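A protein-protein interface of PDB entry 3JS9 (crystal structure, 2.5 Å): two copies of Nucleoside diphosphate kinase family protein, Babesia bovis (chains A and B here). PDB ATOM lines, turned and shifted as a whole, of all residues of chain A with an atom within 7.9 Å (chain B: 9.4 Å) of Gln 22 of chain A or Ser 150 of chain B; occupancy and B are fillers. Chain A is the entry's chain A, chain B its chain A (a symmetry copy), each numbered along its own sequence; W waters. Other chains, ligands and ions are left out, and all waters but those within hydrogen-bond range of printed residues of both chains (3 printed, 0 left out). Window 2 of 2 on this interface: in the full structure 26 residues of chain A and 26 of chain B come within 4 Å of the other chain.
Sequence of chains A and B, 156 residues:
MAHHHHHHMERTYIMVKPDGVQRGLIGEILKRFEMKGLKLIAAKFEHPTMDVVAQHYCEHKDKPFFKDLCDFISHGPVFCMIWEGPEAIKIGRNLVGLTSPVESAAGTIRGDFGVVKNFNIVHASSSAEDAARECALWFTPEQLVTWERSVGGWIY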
ATOM      1  N   VAL A  16      28.807  16.503  30.284  1.00  0.00           N
ATOM      2  CA  VAL A  16      27.856  16.607  29.195  1.00  0.00           C
ATOM      3  C   VAL A  16      26.791  15.551  29.475  1.00  0.00           C
ATOM      4  O   VAL A  16      27.117  14.357  29.596  1.00  0.00           O
ATOM      5  CB  VAL A  16      28.499  16.331  27.827  1.00  0.00           C
ATOM      6  CG1 VAL A  16      27.467  16.535  26.708  1.00  0.00           C
ATOM      7  CG2 VAL A  16      29.690  17.222  27.654  1.00  0.00           C
ATOM      8  N   LYS A  17      25.532  15.985  29.551  1.00  0.00           N
ATOM      9  CA  LYS A  17      24.444  15.105  29.932  1.00  0.00           C
ATOM     10  C   LYS A  17      23.869  14.475  28.672  1.00  0.00           C
ATOM     11  O   LYS A  17      24.252  14.861  27.557  1.00  0.00           O
ATOM     12  CB  LYS A  17      23.367  15.896  30.647  1.00  0.00           C
ATOM     13  CG  LYS A  17      23.758  16.547  31.962  1.00  0.00           C
ATOM     14  CD  LYS A  17      22.547  17.335  32.400  1.00  0.00           C
ATOM     15  CE  LYS A  17      22.811  18.282  33.516  1.00  0.00           C
ATOM     16  NZ  LYS A  17      21.481  18.946  33.761  1.00  0.00           N
ATOM     17  N   PRO A  18      22.923  13.521  28.833  1.00  0.00           N
ATOM     18  CA  PRO A  18      22.462  12.809  27.633  1.00  0.00           C
ATOM     19  C   PRO A  18      21.945  13.690  26.501  1.00  0.00           C
ATOM     20  O   PRO A  18      22.135  13.329  25.329  1.00  0.00           O
ATOM     21  CB  PRO A  18      21.351  11.895  28.173  1.00  0.00           C
ATOM     22  CG  PRO A  18      21.817  11.570  29.573  1.00  0.00           C
ATOM     23  CD  PRO A  18      22.460  12.863  30.079  1.00  0.00           C
ATOM     24  N   ASP A  19      21.274  14.803  26.820  1.00  0.00           N
ATOM     25  CA  ASP A  19      20.741  15.678  25.783  1.00  0.00           C
ATOM     26  C   ASP A  19      21.916  16.339  25.040  1.00  0.00           C
ATOM     27  O   ASP A  19      21.904  16.432  23.802  1.00  0.00           O
ATOM     28  CB  ASP A  19      19.725  16.695  26.352  1.00  0.00           C
ATOM     29  CG  ASP A  19      20.276  17.481  27.554  1.00  0.00           C
ATOM     30  OD1 ASP A  19      20.832  16.847  28.477  1.00  0.00           O
ATOM     31  OD2 ASP A  19      20.175  18.724  27.573  1.00  0.00           O
ATOM     32  N   GLY A  20      22.956  16.752  25.781  1.00  0.00           N
ATOM     33  CA  GLY A  20      24.207  17.219  25.152  1.00  0.00           C
ATOM     34  C   GLY A  20      24.751  16.201  24.139  1.00  0.00           C
ATOM     35  O   GLY A  20      25.123  16.552  22.999  1.00  0.00           O
ATOM     36  N   VAL A  21      24.766  14.926  24.531  1.00  0.00           N
ATOM     37  CA  VAL A  21      25.391  13.912  23.713  1.00  0.00           C
ATOM     38  C   VAL A  21      24.575  13.629  22.470  1.00  0.00           C
ATOM     39  O   VAL A  21      25.137  13.541  21.370  1.00  0.00           O
ATOM     40  CB  VAL A  21      25.649  12.605  24.490  1.00  0.00           C
ATOM     41  CG1 VAL A  21      26.098  11.477  23.540  1.00  0.00           C
ATOM     42  CG2 VAL A  21      26.679  12.839  25.639  1.00  0.00           C
ATOM     43  N   GLN A  22      23.257  13.514  22.639  1.00  0.00           N
ATOM     44  CA  GLN A  22      22.335  13.261  21.518  1.00  0.00           C
ATOM     45  C   GLN A  22      22.377  14.401  20.515  1.00  0.00           C
ATOM     46  O   GLN A  22      22.150  14.208  19.319  1.00  0.00           O
ATOM     47  CB  GLN A  22      20.884  13.066  22.006  1.00  0.00           C
ATOM     48  CG  GLN A  22      20.688  11.853  22.876  1.00  0.00           C
ATOM     49  CD  GLN A  22      20.430  10.574  22.077  1.00  0.00           C
ATOM     50  OE1 GLN A  22      20.258  10.590  20.843  1.00  0.00           O
ATOM     51  NE2 GLN A  22      20.389   9.458  22.784  1.00  0.00           N
ATOM     52  N   ARG A  23      22.669  15.594  20.997  1.00  0.00           N
ATOM     53  CA  ARG A  23      22.645  16.725  20.103  1.00  0.00           C
ATOM     54  C   ARG A  23      23.982  16.985  19.418  1.00  0.00           C
ATOM     55  O   ARG A  23      24.104  17.973  18.662  1.00  0.00           O
ATOM     56  CB  ARG A  23      22.111  17.968  20.829  1.00  0.00           C
ATOM     57  CG  ARG A  23      20.581  17.917  21.032  1.00  0.00           C
ATOM     58  CD  ARG A  23      20.057  19.086  21.880  1.00  0.00           C
ATOM     59  NE  ARG A  23      20.130  20.357  21.156  1.00  0.00           N
ATOM     60  CZ  ARG A  23      20.037  21.556  21.734  1.00  0.00           C
ATOM     61  NH1 ARG A  23      19.845  21.678  23.051  1.00  0.00           N
ATOM     62  NH2 ARG A  23      20.081  22.638  20.983  1.00  0.00           N
ATOM     63  N   GLY A  24      24.961  16.113  19.656  1.00  0.00           N
ATOM     64  CA  GLY A  24      26.300  16.292  19.120  1.00  0.00           C
ATOM     65  C   GLY A  24      27.107  17.482  19.686  1.00  0.00           C
ATOM     66  O   GLY A  24      27.876  18.114  18.960  1.00  0.00           O
ATOM     67  N   LEU A  25      26.994  17.758  20.983  1.00  0.00           N
ATOM     68  CA  LEU A  25      27.728  18.913  21.591  1.00  0.00           C
ATOM     69  C   LEU A  25      28.945  18.585  22.459  1.00  0.00           C
ATOM     70  O   LEU A  25      29.514  19.491  23.114  1.00  0.00           O
ATOM     71  CB  LEU A  25      26.764  19.823  22.374  1.00  0.00           C
ATOM     72  CG  LEU A  25      25.710  20.492  21.460  1.00  0.00           C
ATOM     73  CD1 LEU A  25      24.383  20.772  22.171  1.00  0.00           C
ATOM     74  CD2 LEU A  25      26.279  21.761  20.777  1.00  0.00           C
ATOM     75  N   ILE A  26      29.372  17.324  22.480  1.00  0.00           N
ATOM     76  CA  ILE A  26      30.487  16.969  23.357  1.00  0.00           C
ATOM     77  C   ILE A  26      31.704  17.785  22.980  1.00  0.00           C
ATOM     78  O   ILE A  26      32.349  18.407  23.862  1.00  0.00           O
ATOM     79  CB  ILE A  26      30.878  15.467  23.318  1.00  0.00           C
ATOM     80  CG1 ILE A  26      29.720  14.594  23.828  1.00  0.00           C
ATOM     81  CG2 ILE A  26      32.193  15.229  24.112  1.00  0.00           C
ATOM     82  CD1 ILE A  26      29.840  13.096  23.470  1.00  0.00           C
ATOM     83  N   PHE A  45      33.948   8.961  28.202  1.00  0.00           N
ATOM     84  CA  PHE A  45      32.584   8.718  27.756  1.00  0.00           C
ATOM     85  C   PHE A  45      32.093   7.505  28.579  1.00  0.00           C
ATOM     86  O   PHE A  45      32.826   6.546  28.734  1.00  0.00           O
ATOM     87  CB  PHE A  45      32.636   8.354  26.260  1.00  0.00           C
ATOM     88  CG  PHE A  45      31.301   8.340  25.554  1.00  0.00           C
ATOM     89  CD1 PHE A  45      30.353   9.361  25.761  1.00  0.00           C
ATOM     90  CD2 PHE A  45      31.010   7.329  24.649  1.00  0.00           C
ATOM     91  CE1 PHE A  45      29.154   9.370  25.094  1.00  0.00           C
ATOM     92  CE2 PHE A  45      29.782   7.312  23.956  1.00  0.00           C
ATOM     93  CZ  PHE A  45      28.854   8.341  24.175  1.00  0.00           C
ATOM     94  N   PHE A  72      17.001   9.440  33.999  1.00  0.00           N
ATOM     95  CA  PHE A  72      17.350  10.151  32.796  1.00  0.00           C
ATOM     96  C   PHE A  72      18.871  10.116  32.590  1.00  0.00           C
ATOM     97  O   PHE A  72      19.379   9.884  31.473  1.00  0.00           O
ATOM     98  CB  PHE A  72      16.835  11.588  32.906  1.00  0.00           C
ATOM     99  CG  PHE A  72      17.294  12.475  31.804  1.00  0.00           C
ATOM    100  CD1 PHE A  72      16.783  12.324  30.515  1.00  0.00           C
ATOM    101  CD2 PHE A  72      18.254  13.458  32.047  1.00  0.00           C
ATOM    102  CE1 PHE A  72      17.232  13.151  29.496  1.00  0.00           C
ATOM    103  CE2 PHE A  72      18.692  14.286  31.037  1.00  0.00           C
ATOM    104  CZ  PHE A  72      18.190  14.139  29.764  1.00  0.00           C
ATOM    105  N   HIS A  75      20.324   6.298  32.338  1.00  0.00           N
ATOM    106  CA  HIS A  75      20.110   5.751  30.999  1.00  0.00           C
ATOM    107  C   HIS A  75      21.249   6.169  30.070  1.00  0.00           C
ATOM    108  O   HIS A  75      21.578   5.431  29.131  1.00  0.00           O
ATOM    109  CB  HIS A  75      18.750   6.120  30.413  1.00  0.00           C
ATOM    110  CG  HIS A  75      18.508   5.546  29.050  1.00  0.00           C
ATOM    111  ND1 HIS A  75      18.456   4.188  28.813  1.00  0.00           N
ATOM    112  CD2 HIS A  75      18.305   6.144  27.848  1.00  0.00           C
ATOM    113  CE1 HIS A  75      18.227   3.971  27.528  1.00  0.00           C
ATOM    114  NE2 HIS A  75      18.132   5.142  26.918  1.00  0.00           N
ATOM    115  N   GLY A  76      21.817   7.353  30.343  1.00  0.00           N
ATOM    116  CA  GLY A  76      22.985   7.881  29.663  1.00  0.00           C
ATOM    117  C   GLY A  76      22.786   8.075  28.182  1.00  0.00           C
ATOM    118  O   GLY A  76      21.632   8.179  27.692  1.00  0.00           O
ATOM    119  N   PRO A  77      23.890   8.155  27.439  1.00  0.00           N
ATOM    120  CA  PRO A  77      25.272   8.212  27.888  1.00  0.00           C
ATOM    121  C   PRO A  77      25.632   9.624  28.384  1.00  0.00           C
ATOM    122  O   PRO A  77      24.863  10.571  28.149  1.00  0.00           O
ATOM    123  CB  PRO A  77      26.046   7.908  26.609  1.00  0.00           C
ATOM    124  CG  PRO A  77      25.165   8.376  25.537  1.00  0.00           C
ATOM    125  CD  PRO A  77      23.780   8.186  25.971  1.00  0.00           C
ATOM    126  N   GLU B  34      32.556  14.245  15.537  1.00  0.00           N
ATOM    127  CA  GLU B  34      31.169  14.320  15.931  1.00  0.00           C
ATOM    128  C   GLU B  34      30.338  14.930  14.797  1.00  0.00           C
ATOM    129  O   GLU B  34      29.285  14.378  14.462  1.00  0.00           O
ATOM    130  CB  GLU B  34      31.052  15.117  17.239  1.00  0.00           C
ATOM    131  CG  GLU B  34      29.888  14.802  18.158  1.00  0.00           C
ATOM    132  CD  GLU B  34      30.022  15.558  19.499  1.00  0.00           C
ATOM    133  OE1 GLU B  34      30.928  16.426  19.624  1.00  0.00           O
ATOM    134  OE2 GLU B  34      29.213  15.306  20.433  1.00  0.00           O
ATOM    135  N   MET B  35      30.807  16.037  14.197  1.00  0.00           N
ATOM    136  CA  MET B  35      30.011  16.647  13.126  1.00  0.00           C
ATOM    137  C   MET B  35      29.930  15.740  11.900  1.00  0.00           C
ATOM    138  O   MET B  35      28.931  15.786  11.205  1.00  0.00           O
ATOM    139  CB  MET B  35      30.538  18.023  12.735  1.00  0.00           C
ATOM    140  CG  MET B  35      30.501  19.030  13.853  1.00  0.00           C
ATOM    141  SD  MET B  35      28.818  19.406  14.317  1.00  0.00           S
ATOM    142  CE  MET B  35      28.568  18.181  15.614  1.00  0.00           C
ATOM    143  N   LYS B  39      29.452   7.662  15.126  1.00  0.00           N
ATOM    144  CA  LYS B  39      28.892   7.565  16.459  1.00  0.00           C
ATOM    145  C   LYS B  39      30.005   7.302  17.450  1.00  0.00           C
ATOM    146  O   LYS B  39      30.813   6.388  17.249  1.00  0.00           O
ATOM    147  CB  LYS B  39      27.800   6.470  16.512  1.00  0.00           C
ATOM    148  CG  LYS B  39      27.394   6.160  17.923  1.00  0.00           C
ATOM    149  CD  LYS B  39      26.051   5.547  18.062  1.00  0.00           C
ATOM    150  CE  LYS B  39      26.136   4.035  17.962  1.00  0.00           C
ATOM    151  NZ  LYS B  39      24.951   3.407  18.590  1.00  0.00           N
ATOM    152  N   LEU B  40      30.064   8.100  18.518  1.00  0.00           N
ATOM    153  CA  LEU B  40      31.106   7.892  19.518  1.00  0.00           C
ATOM    154  C   LEU B  40      30.787   6.640  20.328  1.00  0.00           C
ATOM    155  O   LEU B  40      29.656   6.478  20.808  1.00  0.00           O
ATOM    156  CB  LEU B  40      31.229   9.088  20.440  1.00  0.00           C
ATOM    157  CG  LEU B  40      32.360   8.943  21.461  1.00  0.00           C
ATOM    158  CD1 LEU B  40      33.721   8.932  20.745  1.00  0.00           C
ATOM    159  CD2 LEU B  40      32.327  10.069  22.514  1.00  0.00           C
ATOM    160  N   THR B 146      27.262   1.338  24.821  1.00  0.00           N
ATOM    161  CA  THR B 146      26.082   1.063  24.018  1.00  0.00           C
ATOM    162  C   THR B 146      25.060   2.198  24.232  1.00  0.00           C
ATOM    163  O   THR B 146      24.737   2.576  25.377  1.00  0.00           O
ATOM    164  CB  THR B 146      25.474  -0.337  24.375  1.00  0.00           C
ATOM    165  OG1 THR B 146      26.413  -1.373  24.026  1.00  0.00           O
ATOM    166  CG2 THR B 146      24.156  -0.595  23.620  1.00  0.00           C
ATOM    167  N   TRP B 147      24.598   2.780  23.130  1.00  0.00           N
ATOM    168  CA  TRP B 147      23.547   3.791  23.157  1.00  0.00           C
ATOM    169  C   TRP B 147      22.948   3.941  21.781  1.00  0.00           C
ATOM    170  O   TRP B 147      23.514   3.425  20.801  1.00  0.00           O
ATOM    171  CB  TRP B 147      24.067   5.134  23.667  1.00  0.00           C
ATOM    172  CG  TRP B 147      25.089   5.880  22.821  1.00  0.00           C
ATOM    173  CD1 TRP B 147      26.371   5.490  22.544  1.00  0.00           C
ATOM    174  CD2 TRP B 147      24.941   7.200  22.246  1.00  0.00           C
ATOM    175  NE1 TRP B 147      27.011   6.459  21.806  1.00  0.00           N
ATOM    176  CE2 TRP B 147      26.164   7.523  21.623  1.00  0.00           C
ATOM    177  CE3 TRP B 147      23.880   8.124  22.177  1.00  0.00           C
ATOM    178  CZ2 TRP B 147      26.358   8.724  20.924  1.00  0.00           C
ATOM    179  CZ3 TRP B 147      24.070   9.323  21.498  1.00  0.00           C
ATOM    180  CH2 TRP B 147      25.313   9.615  20.882  1.00  0.00           C
ATOM    181  N   GLU B 148      21.812   4.634  21.700  1.00  0.00           N
ATOM    182  CA  GLU B 148      21.146   4.838  20.407  1.00  0.00           C
ATOM    183  C   GLU B 148      20.836   6.314  20.126  1.00  0.00           C
ATOM    184  O   GLU B 148      20.287   7.021  20.985  1.00  0.00           O
ATOM    185  CB  GLU B 148      19.877   3.979  20.314  1.00  0.00           C
ATOM    186  CG  GLU B 148      19.602   3.475  18.896  1.00  0.00           C
ATOM    187  CD  GLU B 148      18.146   3.024  18.669  1.00  0.00           C
ATOM    188  OE1 GLU B 148      17.458   2.669  19.667  1.00  0.00           O
ATOM    189  OE2 GLU B 148      17.694   3.026  17.490  1.00  0.00           O
ATOM    190  N   ARG B 149      21.228   6.784  18.946  1.00  0.00           N
ATOM    191  CA  ARG B 149      20.988   8.165  18.553  1.00  0.00           C
ATOM    192  C   ARG B 149      19.610   8.327  17.964  1.00  0.00           C
ATOM    193  O   ARG B 149      19.287   7.703  16.937  1.00  0.00           O
ATOM    194  CB  ARG B 149      22.023   8.636  17.533  1.00  0.00           C
ATOM    195  CG  ARG B 149      23.306   9.158  18.150  1.00  0.00           C
ATOM    196  CD  ARG B 149      24.297   9.629  17.086  1.00  0.00           C
ATOM    197  NE  ARG B 149      24.453   8.655  15.999  1.00  0.00           N
ATOM    198  CZ  ARG B 149      25.372   8.750  15.048  1.00  0.00           C
ATOM    199  NH1 ARG B 149      26.228   9.773  15.055  1.00  0.00           N
ATOM    200  NH2 ARG B 149      25.458   7.821  14.112  1.00  0.00           N
ATOM    201  N   SER B 150      18.795   9.166  18.594  1.00  0.00           N
ATOM    202  CA  SER B 150      17.504   9.520  18.013  1.00  0.00           C
ATOM    203  C   SER B 150      17.668  10.013  16.569  1.00  0.00           C
ATOM    204  O   SER B 150      16.839   9.710  15.723  1.00  0.00           O
ATOM    205  CB  SER B 150      16.843  10.617  18.830  1.00  0.00           C
ATOM    206  OG  SER B 150      16.592  10.188  20.150  1.00  0.00           O
ATOM    207  N   VAL B 151      18.742  10.763  16.291  1.00  0.00           N
ATOM    208  CA  VAL B 151      18.990  11.320  14.969  1.00  0.00           C
ATOM    209  C   VAL B 151      19.685  10.356  13.982  1.00  0.00           C
ATOM    210  O   VAL B 151      19.729  10.612  12.769  1.00  0.00           O
ATOM    211  CB  VAL B 151      19.766  12.659  15.088  1.00  0.00           C
ATOM    212  CG1 VAL B 151      21.258  12.426  15.227  1.00  0.00           C
ATOM    213  CG2 VAL B 151      19.466  13.548  13.922  1.00  0.00           C
ATOM    214  N   GLY B 152      20.186   9.236  14.515  1.00  0.00           N
ATOM    215  CA  GLY B 152      20.988   8.262  13.779  1.00  0.00           C
ATOM    216  C   GLY B 152      20.519   7.860  12.408  1.00  0.00           C
ATOM    217  O   GLY B 152      21.346   7.699  11.510  1.00  0.00           O
ATOM    218  N   GLY B 153      19.200   7.713  12.239  1.00  0.00           N
ATOM    219  CA  GLY B 153      18.589   7.204  11.021  1.00  0.00           C
ATOM    220  C   GLY B 153      18.629   8.203   9.881  1.00  0.00           C
ATOM    221  O   GLY B 153      18.341   7.851   8.727  1.00  0.00           O
ATOM    222  N   TRP B 154      18.947   9.455  10.205  1.00  0.00           N
ATOM    223  CA  TRP B 154      19.225  10.470   9.209  1.00  0.00           C
ATOM    224  C   TRP B 154      20.724  10.587   8.904  1.00  0.00           C
ATOM    225  O   TRP B 154      21.102  11.451   8.110  1.00  0.00           O
ATOM    226  CB  TRP B 154      18.702  11.846   9.653  1.00  0.00           C
ATOM    227  CG  TRP B 154      17.264  11.871   9.998  1.00  0.00           C
ATOM    228  CD1 TRP B 154      16.724  11.724  11.235  1.00  0.00           C
ATOM    229  CD2 TRP B 154      16.167  12.027   9.092  1.00  0.00           C
ATOM    230  NE1 TRP B 154      15.354  11.780  11.163  1.00  0.00           N
ATOM    231  CE2 TRP B 154      14.983  11.971   9.860  1.00  0.00           C
ATOM    232  CE3 TRP B 154      16.066  12.188   7.704  1.00  0.00           C
ATOM    233  CZ2 TRP B 154      13.706  12.093   9.289  1.00  0.00           C
ATOM    234  CZ3 TRP B 154      14.773  12.311   7.131  1.00  0.00           C
ATOM    235  CH2 TRP B 154      13.623  12.259   7.929  1.00  0.00           C
ATOM    236  N   ILE B 155      21.579   9.753   9.516  1.00  0.00           N
ATOM    237  CA  ILE B 155      23.022   9.820   9.227  1.00  0.00           C
ATOM    238  C   ILE B 155      23.428   8.614   8.384  1.00  0.00           C
ATOM    239  O   ILE B 155      24.129   8.755   7.371  1.00  0.00           O
ATOM    240  CB  ILE B 155      23.883  10.002  10.496  1.00  0.00           C
ATOM    241  CG1 ILE B 155      23.401  11.218  11.325  1.00  0.00           C
ATOM    242  CG2 ILE B 155      25.345  10.199  10.125  1.00  0.00           C
ATOM    243  CD1 ILE B 155      24.063  11.370  12.729  1.00  0.00           C
ATOM    244  N   TYR B 156      22.939   7.435   8.771  1.00  0.00           N
ATOM    245  CA  TYR B 156      23.104   6.202   7.989  1.00  0.00           C
ATOM    246  C   TYR B 156      22.165   5.108   8.485  1.00  0.00           C
ATOM    247  O   TYR B 156      22.049   4.066   7.805  1.00  0.00           O
ATOM    248  CB  TYR B 156      24.559   5.691   8.021  1.00  0.00           C
ATOM    249  CG  TYR B 156      25.175   5.540   9.413  1.00  0.00           C
ATOM    250  CD1 TYR B 156      26.048   6.506   9.925  1.00  0.00           C
ATOM    251  CD2 TYR B 156      24.905   4.412  10.206  1.00  0.00           C
ATOM    252  CE1 TYR B 156      26.625   6.358  11.205  1.00  0.00           C
ATOM    253  CE2 TYR B 156      25.473   4.253  11.472  1.00  0.00           C
ATOM    254  CZ  TYR B 156      26.326   5.238  11.972  1.00  0.00           C
ATOM    255  OH  TYR B 156      26.904   5.060  13.232  1.00  0.00           O
ATOM    256  OXT TYR B 156      21.540   5.225   9.562  1.00  0.00           O
HETATM  257  O   HOH W   1      27.696  12.934  20.078  1.00  0.00           O
HETATM  258  O   HOH W   2      30.469  19.208  19.259  1.00  0.00           O
HETATM  259  O   HOH W   3      20.279  12.217  18.718  1.00  0.00           O
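Printed residues of chain B within 4 Å of Gln 22 of chain A: Trp 147 (3.8 Å), Glu 148 (3.0 Å), Arg 149 (3.4 Å) and Ser 150 (3.0 Å).
Of chain A, only Gln 22 (3.0 Å) comes within 4 Å of Ser 150 of chain B.
No residue of chain B comes within 4 Å of Gly 20 of chain A.
Of chain B, only Trp 147 (3.3 Å) comes within 4 Å of Val 21 of chain A.
Printed residues of chain B within 4 Å of Ile 26 of chain A: Glu 34 (2.9 Å).
Printed residues of chain B within 4 Å of Phe 45 of chain A: Leu 40 (3.3 Å) and Trp 147 (3.5 Å).
The nearest residue of chain B that does not touch Gln 22 of chain A is Val 151 of chain B (4.6 Å).
The nearest printed residue of chain A that does not touch Ser 150 of chain B is Arg 23 of chain A (7.9 Å).
No position is printed for both chains.
Of the 12 pairs that touch across the chains among the printed residues, none has its exchanged pair printed and touching as well.
Printed residues of chain A that touch a printed residue of chain B: Val 21, Gln 22, Gly 24, Leu 25, Ile 26, Phe 45 and Pro 77.
Hydrophobic or aromatic side chains of chain A within 4 Å of the printed part of chain B: Val 21, Ile 26, Phe 45 and Pro 77.
Printed residues of chain B that touch a printed residue of chain A: Glu 34, Met 35, Leu 40, Trp 147, Glu 148, Arg 149 and Ser 150.
Hydrophobic or aromatic side chains of chain B that line the printed part of chain A: Met 35, Leu 40 and Trp 147.
Along chain B the printed residues that touch a printed residue of chain A span positions 34 to 150.
Among the printed residues, no Asp or Glu carboxylate lies within 4 Å of a Lys or Arg side-chain nitrogen of the other chain.
Trp 147 of chain B touches Val 21 of chain A.
Trp 147 of chain B touches Gln 22 of chain A.
Gln 22 of chain A touches Arg 149 of chain B (OE1 to CA, 3.4 Å).
O of Gly 24 of chain A touches CE of Met 35 of chain B, 3.4 Å away.
CE2 of Phe 45 of chain A touches O of Leu 40 of chain B, at 3.3 Å.
Phe 45 of chain A touches Trp 147 of chain B (CZ to NE1, 3.5 Å).
CG of Pro 77 of chain A touches CD2 of Trp 147 of chain B (3.5 Å).
OE2 of Glu 34 of chain B sits close to O of Gly 24 of chain A (3.4 Å).
The side-chain amide oxygen of Gln 22 of chain A is in hydrogen-bond range of the backbone NH of Ser 150 of chain B (3.0 Å).
The backbone carbonyl oxygen (O) of Glu 148 of chain B lies within hydrogen-bond range of the side-chain amide nitrogen (NE2) of Gln 22 of chain A (3.0 Å).
N of Leu 25 of chain A lies within hydrogen-bond range of OE2 of Glu 34 of chain B (3.4 Å).
N of Ile 26 of chain A is in hydrogen-bond range of OE2 of Glu 34 of chain B (2.9 Å).
OH of Tyr 156 of chain B is in hydrogen-bond range of NH2 of Arg 149 of chain B, at 3.2 Å.
O of Trp 147 of chain B is in hydrogen-bond range of NZ of Lys 39 of chain B (2.6 Å).
The backbone carbonyl oxygen (O) of Gly 20 of chain A lies within hydrogen-bond range of the backbone NH (N) of Leu 25 of chain A (3.0 Å).
The backbone carbonyl oxygen of Leu 40 of chain B is in hydrogen-bond range of the indole nitrogen of Trp 147 of chain B (2.8 Å).
Water W3 lies within hydrogen-bond range of the side-chain amide oxygen of Gln 22 of chain A (2.7 Å), the backbone NH of Val 151 of chain B (3.2 Å) and the backbone NH of Ser 150 of chain B (3.4 Å).
Water W2 lies within hydrogen-bond range of O of Gly 24 of chain A (2.8 Å) and OE1 of Glu 34 of chain B (2.8 Å).
Water W1 bridges the side-chain carboxylate of Glu 34 of chain B (2.8 Å) and the backbone carbonyl oxygen of Val 21 of chain A (2.9 Å).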
